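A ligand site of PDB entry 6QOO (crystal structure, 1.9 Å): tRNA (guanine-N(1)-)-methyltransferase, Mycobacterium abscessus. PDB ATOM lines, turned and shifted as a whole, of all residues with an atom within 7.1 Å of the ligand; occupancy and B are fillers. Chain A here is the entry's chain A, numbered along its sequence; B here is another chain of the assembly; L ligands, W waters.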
ATOM      1  N   VAL A  84     -13.242 -17.892  -1.916  1.00  0.00           N
ATOM      2  CA  VAL A  84     -12.901 -18.796  -0.810  1.00  0.00           C
ATOM      3  C   VAL A  84     -13.841 -18.557   0.358  1.00  0.00           C
ATOM      4  O   VAL A  84     -13.684 -17.568   1.059  1.00  0.00           O
ATOM      5  CB  VAL A  84     -11.439 -18.628  -0.350  1.00  0.00           C
ATOM      6  CG1 VAL A  84     -11.084 -19.694   0.699  1.00  0.00           C
ATOM      7  CG2 VAL A  84     -10.476 -18.711  -1.549  1.00  0.00           C
ATOM      8  N   PRO A  85     -14.846 -19.423   0.554  1.00  0.00           N
ATOM      9  CA  PRO A  85     -15.744 -19.194   1.688  1.00  0.00           C
ATOM     10  C   PRO A  85     -15.067 -19.528   3.020  1.00  0.00           C
ATOM     11  O   PRO A  85     -14.528 -20.608   3.184  1.00  0.00           O
ATOM     12  CB  PRO A  85     -16.908 -20.154   1.421  1.00  0.00           C
ATOM     13  CG  PRO A  85     -16.845 -20.413  -0.064  1.00  0.00           C
ATOM     14  CD  PRO A  85     -15.391 -20.424  -0.376  1.00  0.00           C
ATOM     15  N   THR A  86     -15.167 -18.760   4.022  1.00  0.00           N
ATOM     16  CA  THR A  86     -14.478 -18.744   5.295  1.00  0.00           C
ATOM     17  C   THR A  86     -15.145 -17.720   6.194  1.00  0.00           C
ATOM     18  O   THR A  86     -15.578 -16.678   5.706  1.00  0.00           O
ATOM     19  CB  THR A  86     -12.989 -18.395   5.133  1.00  0.00           C
ATOM     20  OG1 THR A  86     -12.317 -18.597   6.384  1.00  0.00           O
ATOM     21  CG2 THR A  86     -12.825 -16.934   4.719  1.00  0.00           C
ATOM     22  N   PRO A  87     -15.279 -18.354   7.501  1.00  0.00           N
ATOM     23  CA  PRO A  87     -15.879 -17.470   8.520  1.00  0.00           C
ATOM     24  C   PRO A  87     -14.973 -16.278   8.848  1.00  0.00           C
ATOM     25  O   PRO A  87     -15.410 -15.368   9.524  1.00  0.00           O
ATOM     26  CB  PRO A  87     -16.050 -18.398   9.745  1.00  0.00           C
ATOM     27  CG  PRO A  87     -15.042 -19.490   9.541  1.00  0.00           C
ATOM     28  CD  PRO A  87     -14.967 -19.694   8.038  1.00  0.00           C
ATOM     29  N   ALA A  88     -13.729 -16.293   8.367  1.00  0.00           N
ATOM     30  CA  ALA A  88     -12.843 -15.154   8.570  1.00  0.00           C
ATOM     31  C   ALA A  88     -12.846 -14.165   7.398  1.00  0.00           C
ATOM     32  O   ALA A  88     -11.980 -13.300   7.318  1.00  0.00           O
ATOM     33  CB  ALA A  88     -11.415 -15.642   8.829  1.00  0.00           C
ATOM     34  N   GLY A  89     -13.805 -14.289   6.492  1.00  0.00           N
ATOM     35  CA  GLY A  89     -13.779 -13.527   5.252  1.00  0.00           C
ATOM     36  C   GLY A  89     -14.427 -12.155   5.342  1.00  0.00           C
ATOM     37  O   GLY A  89     -15.005 -11.797   6.360  1.00  0.00           O
ATOM     38  N   GLY A 111     -13.153 -25.318   1.593  1.00  0.00           N
ATOM     39  CA  GLY A 111     -12.280 -25.979   2.557  1.00  0.00           C
ATOM     40  C   GLY A 111     -12.881 -26.052   3.946  1.00  0.00           C
ATOM     41  O   GLY A 111     -13.894 -25.419   4.225  1.00  0.00           O
ATOM     42  N   ARG A 112     -12.254 -26.822   4.828  1.00  0.00           N
ATOM     43  CA  ARG A 112     -12.715 -26.867   6.218  1.00  0.00           C
ATOM     44  C   ARG A 112     -12.523 -25.500   6.886  1.00  0.00           C
ATOM     45  O   ARG A 112     -11.672 -24.712   6.477  1.00  0.00           O
ATOM     46  CB  ARG A 112     -11.976 -27.949   7.000  1.00  0.00           C
ATOM     47  CG  ARG A 112     -10.471 -27.831   6.974  1.00  0.00           C
ATOM     48  CD  ARG A 112      -9.856 -29.078   7.622  1.00  0.00           C
ATOM     49  NE  ARG A 112     -10.343 -29.259   8.992  1.00  0.00           N
ATOM     50  CZ  ARG A 112     -10.454 -30.430   9.612  1.00  0.00           C
ATOM     51  NH1 ARG A 112     -10.901 -30.487  10.855  1.00  0.00           N
ATOM     52  NH2 ARG A 112     -10.133 -31.554   8.982  1.00  0.00           N
ATOM     53  N   TYR A 113     -13.305 -25.218   7.922  1.00  0.00           N
ATOM     54  CA  TYR A 113     -13.374 -23.832   8.425  1.00  0.00           C
ATOM     55  C   TYR A 113     -12.067 -23.398   9.107  1.00  0.00           C
ATOM     56  O   TYR A 113     -11.775 -22.196   9.171  1.00  0.00           O
ATOM     57  CB  TYR A 113     -14.545 -23.665   9.388  1.00  0.00           C
ATOM     58  CG  TYR A 113     -14.239 -24.077  10.798  1.00  0.00           C
ATOM     59  CD1 TYR A 113     -14.413 -25.399  11.199  1.00  0.00           C
ATOM     60  CD2 TYR A 113     -13.756 -23.165  11.734  1.00  0.00           C
ATOM     61  CE1 TYR A 113     -14.134 -25.795  12.500  1.00  0.00           C
ATOM     62  CE2 TYR A 113     -13.469 -23.557  13.038  1.00  0.00           C
ATOM     63  CZ  TYR A 113     -13.663 -24.867  13.412  1.00  0.00           C
ATOM     64  OH  TYR A 113     -13.368 -25.254  14.689  1.00  0.00           O
ATOM     65  N   GLU A 114     -11.287 -24.350   9.622  1.00  0.00           N
ATOM     66  CA  GLU A 114     -10.009 -24.021  10.243  1.00  0.00           C
ATOM     67  C   GLU A 114      -9.111 -23.373   9.211  1.00  0.00           C
ATOM     68  O   GLU A 114      -8.255 -22.545   9.531  1.00  0.00           O
ATOM     69  CB  GLU A 114      -9.319 -25.253  10.833  1.00  0.00           C
ATOM     70  CG  GLU A 114     -10.137 -25.970  11.910  1.00  0.00           C
ATOM     71  CD  GLU A 114     -10.976 -27.098  11.343  1.00  0.00           C
ATOM     72  OE1 GLU A 114     -11.401 -27.003  10.165  1.00  0.00           O
ATOM     73  OE2 GLU A 114     -11.217 -28.081  12.070  1.00  0.00           O
ATOM     74  N   VAL A 133     -14.507 -14.724   1.648  1.00  0.00           N
ATOM     75  CA  VAL A 133     -15.773 -14.112   2.057  1.00  0.00           C
ATOM     76  C   VAL A 133     -16.510 -15.013   3.028  1.00  0.00           C
ATOM     77  O   VAL A 133     -16.367 -16.237   2.987  1.00  0.00           O
ATOM     78  CB  VAL A 133     -16.697 -13.837   0.860  1.00  0.00           C
ATOM     79  CG1 VAL A 133     -16.065 -12.800  -0.092  1.00  0.00           C
ATOM     80  CG2 VAL A 133     -17.004 -15.148   0.099  1.00  0.00           C
ATOM     81  N   SER A 134     -17.282 -14.383   3.915  1.00  0.00           N
ATOM     82  CA  SER A 134     -18.152 -15.099   4.842  1.00  0.00           C
ATOM     83  C   SER A 134     -19.593 -14.828   4.488  1.00  0.00           C
ATOM     84  O   SER A 134     -19.948 -13.690   4.261  1.00  0.00           O
ATOM     85  CB  SER A 134     -17.889 -14.657   6.279  1.00  0.00           C
ATOM     86  OG  SER A 134     -18.872 -15.194   7.123  1.00  0.00           O
ATOM     87  N   ILE A 135     -20.423 -15.861   4.459  1.00  0.00           N
ATOM     88  CA  ILE A 135     -21.847 -15.628   4.179  1.00  0.00           C
ATOM     89  C   ILE A 135     -22.668 -15.307   5.454  1.00  0.00           C
ATOM     90  O   ILE A 135     -23.873 -15.041   5.371  1.00  0.00           O
ATOM     91  CB  ILE A 135     -22.490 -16.830   3.482  1.00  0.00           C
ATOM     92  CG1 ILE A 135     -22.382 -18.080   4.372  1.00  0.00           C
ATOM     93  CG2 ILE A 135     -21.883 -16.995   2.076  1.00  0.00           C
ATOM     94  CD1 ILE A 135     -23.419 -19.149   4.053  1.00  0.00           C
ATOM     95  N   GLY A 136     -22.019 -15.338   6.611  1.00  0.00           N
ATOM     96  CA  GLY A 136     -22.699 -14.998   7.864  1.00  0.00           C
ATOM     97  C   GLY A 136     -21.862 -15.344   9.077  1.00  0.00           C
ATOM     98  O   GLY A 136     -20.831 -16.013   8.962  1.00  0.00           O
ATOM     99  N   ASP A 137     -22.292 -14.903  10.255  1.00  0.00           N
ATOM    100  CA  ASP A 137     -21.506 -15.068  11.464  1.00  0.00           C
ATOM    101  C   ASP A 137     -21.864 -16.339  12.220  1.00  0.00           C
ATOM    102  O   ASP A 137     -22.481 -16.329  13.303  1.00  0.00           O
ATOM    103  CB  ASP A 137     -21.653 -13.846  12.383  1.00  0.00           C
ATOM    104  CG  ASP A 137     -20.855 -12.679  11.885  1.00  0.00           C
ATOM    105  OD1 ASP A 137     -19.814 -12.903  11.196  1.00  0.00           O
ATOM    106  OD2 ASP A 137     -21.234 -11.537  12.165  1.00  0.00           O
ATOM    107  N   TYR A 138     -21.420 -17.436  11.638  1.00  0.00           N
ATOM    108  CA  TYR A 138     -21.615 -18.758  12.190  1.00  0.00           C
ATOM    109  C   TYR A 138     -20.562 -19.626  11.539  1.00  0.00           C
ATOM    110  O   TYR A 138     -20.033 -19.289  10.471  1.00  0.00           O
ATOM    111  CB  TYR A 138     -23.021 -19.311  11.915  1.00  0.00           C
ATOM    112  CG  TYR A 138     -23.559 -18.918  10.574  1.00  0.00           C
ATOM    113  CD1 TYR A 138     -23.121 -19.556   9.408  1.00  0.00           C
ATOM    114  CD2 TYR A 138     -24.484 -17.884  10.452  1.00  0.00           C
ATOM    115  CE1 TYR A 138     -23.601 -19.179   8.157  1.00  0.00           C
ATOM    116  CE2 TYR A 138     -24.968 -17.502   9.208  1.00  0.00           C
ATOM    117  CZ  TYR A 138     -24.524 -18.151   8.072  1.00  0.00           C
ATOM    118  OH  TYR A 138     -24.990 -17.742   6.837  1.00  0.00           O
ATOM    119  N   VAL A 139     -20.241 -20.717  12.202  1.00  0.00           N
ATOM    120  CA  VAL A 139     -19.269 -21.658  11.681  1.00  0.00           C
ATOM    121  C   VAL A 139     -19.978 -22.884  11.132  1.00  0.00           C
ATOM    122  O   VAL A 139     -20.915 -23.393  11.749  1.00  0.00           O
ATOM    123  CB  VAL A 139     -18.289 -22.082  12.785  1.00  0.00           C
ATOM    124  CG1 VAL A 139     -17.311 -23.164  12.260  1.00  0.00           C
ATOM    125  CG2 VAL A 139     -17.536 -20.857  13.280  1.00  0.00           C
ATOM    126  N   LEU A 140     -19.492 -23.327   9.971  1.00  0.00           N
ATOM    127  CA  LEU A 140     -19.849 -24.599   9.349  1.00  0.00           C
ATOM    128  C   LEU A 140     -18.591 -25.472   9.340  1.00  0.00           C
ATOM    129  O   LEU A 140     -17.478 -24.945   9.411  1.00  0.00           O
ATOM    130  CB  LEU A 140     -20.349 -24.381   7.905  1.00  0.00           C
ATOM    131  CG  LEU A 140     -21.316 -23.219   7.677  1.00  0.00           C
ATOM    132  CD1 LEU A 140     -21.582 -22.972   6.174  1.00  0.00           C
ATOM    133  CD2 LEU A 140     -22.617 -23.454   8.418  1.00  0.00           C
ATOM    134  N   ASN A 141     -18.738 -26.782   9.237  1.00  0.00           N
ATOM    135  CA  ASN A 141     -17.571 -27.657   9.186  1.00  0.00           C
ATOM    136  C   ASN A 141     -16.682 -27.314   7.980  1.00  0.00           C
ATOM    137  O   ASN A 141     -15.459 -27.369   8.062  1.00  0.00           O
ATOM    138  CB  ASN A 141     -17.991 -29.120   9.136  1.00  0.00           C
ATOM    139  CG  ASN A 141     -17.962 -29.769  10.512  1.00  0.00           C
ATOM    140  OD1 ASN A 141     -18.017 -29.073  11.533  1.00  0.00           O
ATOM    141  ND2 ASN A 141     -17.877 -31.096  10.551  1.00  0.00           N
ATOM    142  N   GLY A 142     -17.319 -26.930   6.884  1.00  0.00           N
ATOM    143  CA  GLY A 142     -16.595 -26.603   5.664  1.00  0.00           C
ATOM    144  C   GLY A 142     -17.382 -25.588   4.851  1.00  0.00           C
ATOM    145  O   GLY A 142     -18.516 -25.252   5.179  1.00  0.00           O
ATOM    146  N   GLY A 143     -16.757 -25.096   3.782  1.00  0.00           N
ATOM    147  CA  GLY A 143     -17.361 -24.071   2.943  1.00  0.00           C
ATOM    148  C   GLY A 143     -18.403 -24.561   1.960  1.00  0.00           C
ATOM    149  O   GLY A 143     -18.937 -23.771   1.182  1.00  0.00           O
ATOM    150  N   GLU A 144     -18.719 -25.854   1.995  1.00  0.00           N
ATOM    151  CA  GLU A 144     -19.612 -26.449   0.989  1.00  0.00           C
ATOM    152  C   GLU A 144     -21.007 -25.811   0.969  1.00  0.00           C
ATOM    153  O   GLU A 144     -21.478 -25.385  -0.087  1.00  0.00           O
ATOM    154  CB  GLU A 144     -19.746 -27.962   1.241  1.00  0.00           C
ATOM    155  CG  GLU A 144     -18.635 -28.821   0.646  1.00  0.00           C
ATOM    156  CD  GLU A 144     -17.311 -28.698   1.379  1.00  0.00           C
ATOM    157  OE1 GLU A 144     -17.297 -28.251   2.548  1.00  0.00           O
ATOM    158  OE2 GLU A 144     -16.273 -29.058   0.766  1.00  0.00           O
ATOM    159  N   ALA A 146     -21.868 -22.993   2.079  1.00  0.00           N
ATOM    160  CA  ALA A 146     -21.714 -21.575   1.753  1.00  0.00           C
ATOM    161  C   ALA A 146     -21.549 -21.402   0.263  1.00  0.00           C
ATOM    162  O   ALA A 146     -21.998 -20.426  -0.306  1.00  0.00           O
ATOM    163  CB  ALA A 146     -20.545 -20.973   2.492  1.00  0.00           C
ATOM    164  N   ALA A 147     -20.886 -22.375  -0.378  1.00  0.00           N
ATOM    165  CA  ALA A 147     -20.763 -22.375  -1.823  1.00  0.00           C
ATOM    166  C   ALA A 147     -22.122 -22.476  -2.496  1.00  0.00           C
ATOM    167  O   ALA A 147     -22.347 -21.845  -3.516  1.00  0.00           O
ATOM    168  CB  ALA A 147     -19.854 -23.550  -2.284  1.00  0.00           C
ATOM    169  N   ILE A 150     -23.802 -19.004  -2.132  1.00  0.00           N
ATOM    170  CA  ILE A 150     -23.184 -18.064  -3.066  1.00  0.00           C
ATOM    171  C   ILE A 150     -23.650 -18.333  -4.501  1.00  0.00           C
ATOM    172  O   ILE A 150     -24.033 -17.412  -5.230  1.00  0.00           O
ATOM    173  CB  ILE A 150     -21.644 -18.117  -2.971  1.00  0.00           C
ATOM    174  CG1 ILE A 150     -21.188 -17.534  -1.614  1.00  0.00           C
ATOM    175  CG2 ILE A 150     -21.000 -17.374  -4.104  1.00  0.00           C
ATOM    176  CD1 ILE A 150     -19.693 -17.656  -1.364  1.00  0.00           C
ATOM    177  N   ARG B 156     -23.359 -29.605  13.856  1.00  0.00           N
ATOM    178  CA  ARG B 156     -21.980 -29.738  14.337  1.00  0.00           C
ATOM    179  C   ARG B 156     -21.856 -29.379  15.818  1.00  0.00           C
ATOM    180  O   ARG B 156     -20.829 -29.650  16.443  1.00  0.00           O
ATOM    181  CB  ARG B 156     -21.024 -28.887  13.492  1.00  0.00           C
ATOM    182  CG  ARG B 156     -21.313 -27.396  13.505  1.00  0.00           C
ATOM    183  CD  ARG B 156     -20.285 -26.642  12.675  1.00  0.00           C
ATOM    184  NE  ARG B 156     -18.923 -26.808  13.184  1.00  0.00           N
ATOM    185  CZ  ARG B 156     -18.398 -26.058  14.147  1.00  0.00           C
ATOM    186  NH1 ARG B 156     -19.123 -25.120  14.749  1.00  0.00           N
ATOM    187  NH2 ARG B 156     -17.145 -26.260  14.552  1.00  0.00           N
HETATM  188  N1  LIG L   1     -19.450 -18.403   7.569  1.00  0.00           N
HETATM  189  C1  LIG L   1     -18.827 -19.179   6.557  1.00  0.00           C
HETATM  190  S1  LIG L   1     -18.774 -18.683   4.960  1.00  0.00           S
HETATM  191  C2  LIG L   1     -18.210 -20.486   6.936  1.00  0.00           C
HETATM  192  C3  LIG L   1     -17.576 -21.366   6.077  1.00  0.00           C
HETATM  193  C4  LIG L   1     -17.142 -22.443   6.835  1.00  0.00           C
HETATM  194  N2  LIG L   1     -17.507 -22.214   8.114  1.00  0.00           N
HETATM  195  O1  LIG L   1     -18.161 -20.999   8.188  1.00  0.00           O
HETATM  196  O   HOH W   1     -14.109 -22.570   5.168  1.00  0.00           O
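A nitrogen (N2) of the ligand sits at hydrogen-bond distance from the backbone NH of Leu 140 (2.9 Å).
O of Tyr 138 lies within hydrogen-bond range of N1 of the ligand (3.1 Å).
The backbone carbonyl oxygen (O) of Gly 136 sits at hydrogen-bond distance from a nitrogen (N1) of the ligand (3.1 Å).
OG of Ser 134 sits at hydrogen-bond distance from N1 of the ligand (3.3 Å).
S1 of the ligand sits close to N of Ile 135.
N of Thr 86 sits close to S1 of the ligand.
The side-chain hydroxyl (OH) of Tyr 138 sits at hydrogen-bond distance from the backbone carbonyl oxygen (O) of Ile 135 (3.3 Å).
O of Gly 136 lies within hydrogen-bond range of OG of Ser 134 (2.8 Å).
N of Ser 134 lies close to O of Thr 86.
N of Tyr 113 is in hydrogen-bond range of O of Asn 141 (3.0 Å).
O of Val 133 sits at hydrogen-bond distance from N of Thr 86, 3.0 Å away.
OG1 of Thr 86 sits close to N of Ala 88 (3.4 Å).
The backbone NH (N) of Val 133 is in hydrogen-bond range of the backbone carbonyl oxygen (O) of Val 84, at 3.0 Å.
Residues that only touch the ligand: Pro 87 (3.5 Å), Tyr 113 (3.5 Å), Val 133 (3.96 Å), Val 139 (3.7 Å), Gly 142 (3.5 Å) and Ala 146 (3.8 Å).
Within 4 Å of the ligand: Thr 86, Pro 87, Tyr 113, Val 133, Ser 134, Ile 135, Gly 136, Tyr 138, Val 139, Leu 140, Gly 142 and Ala 146.
The nearest printed residue that does not touch the ligand is Gly 143 (4.1 Å).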
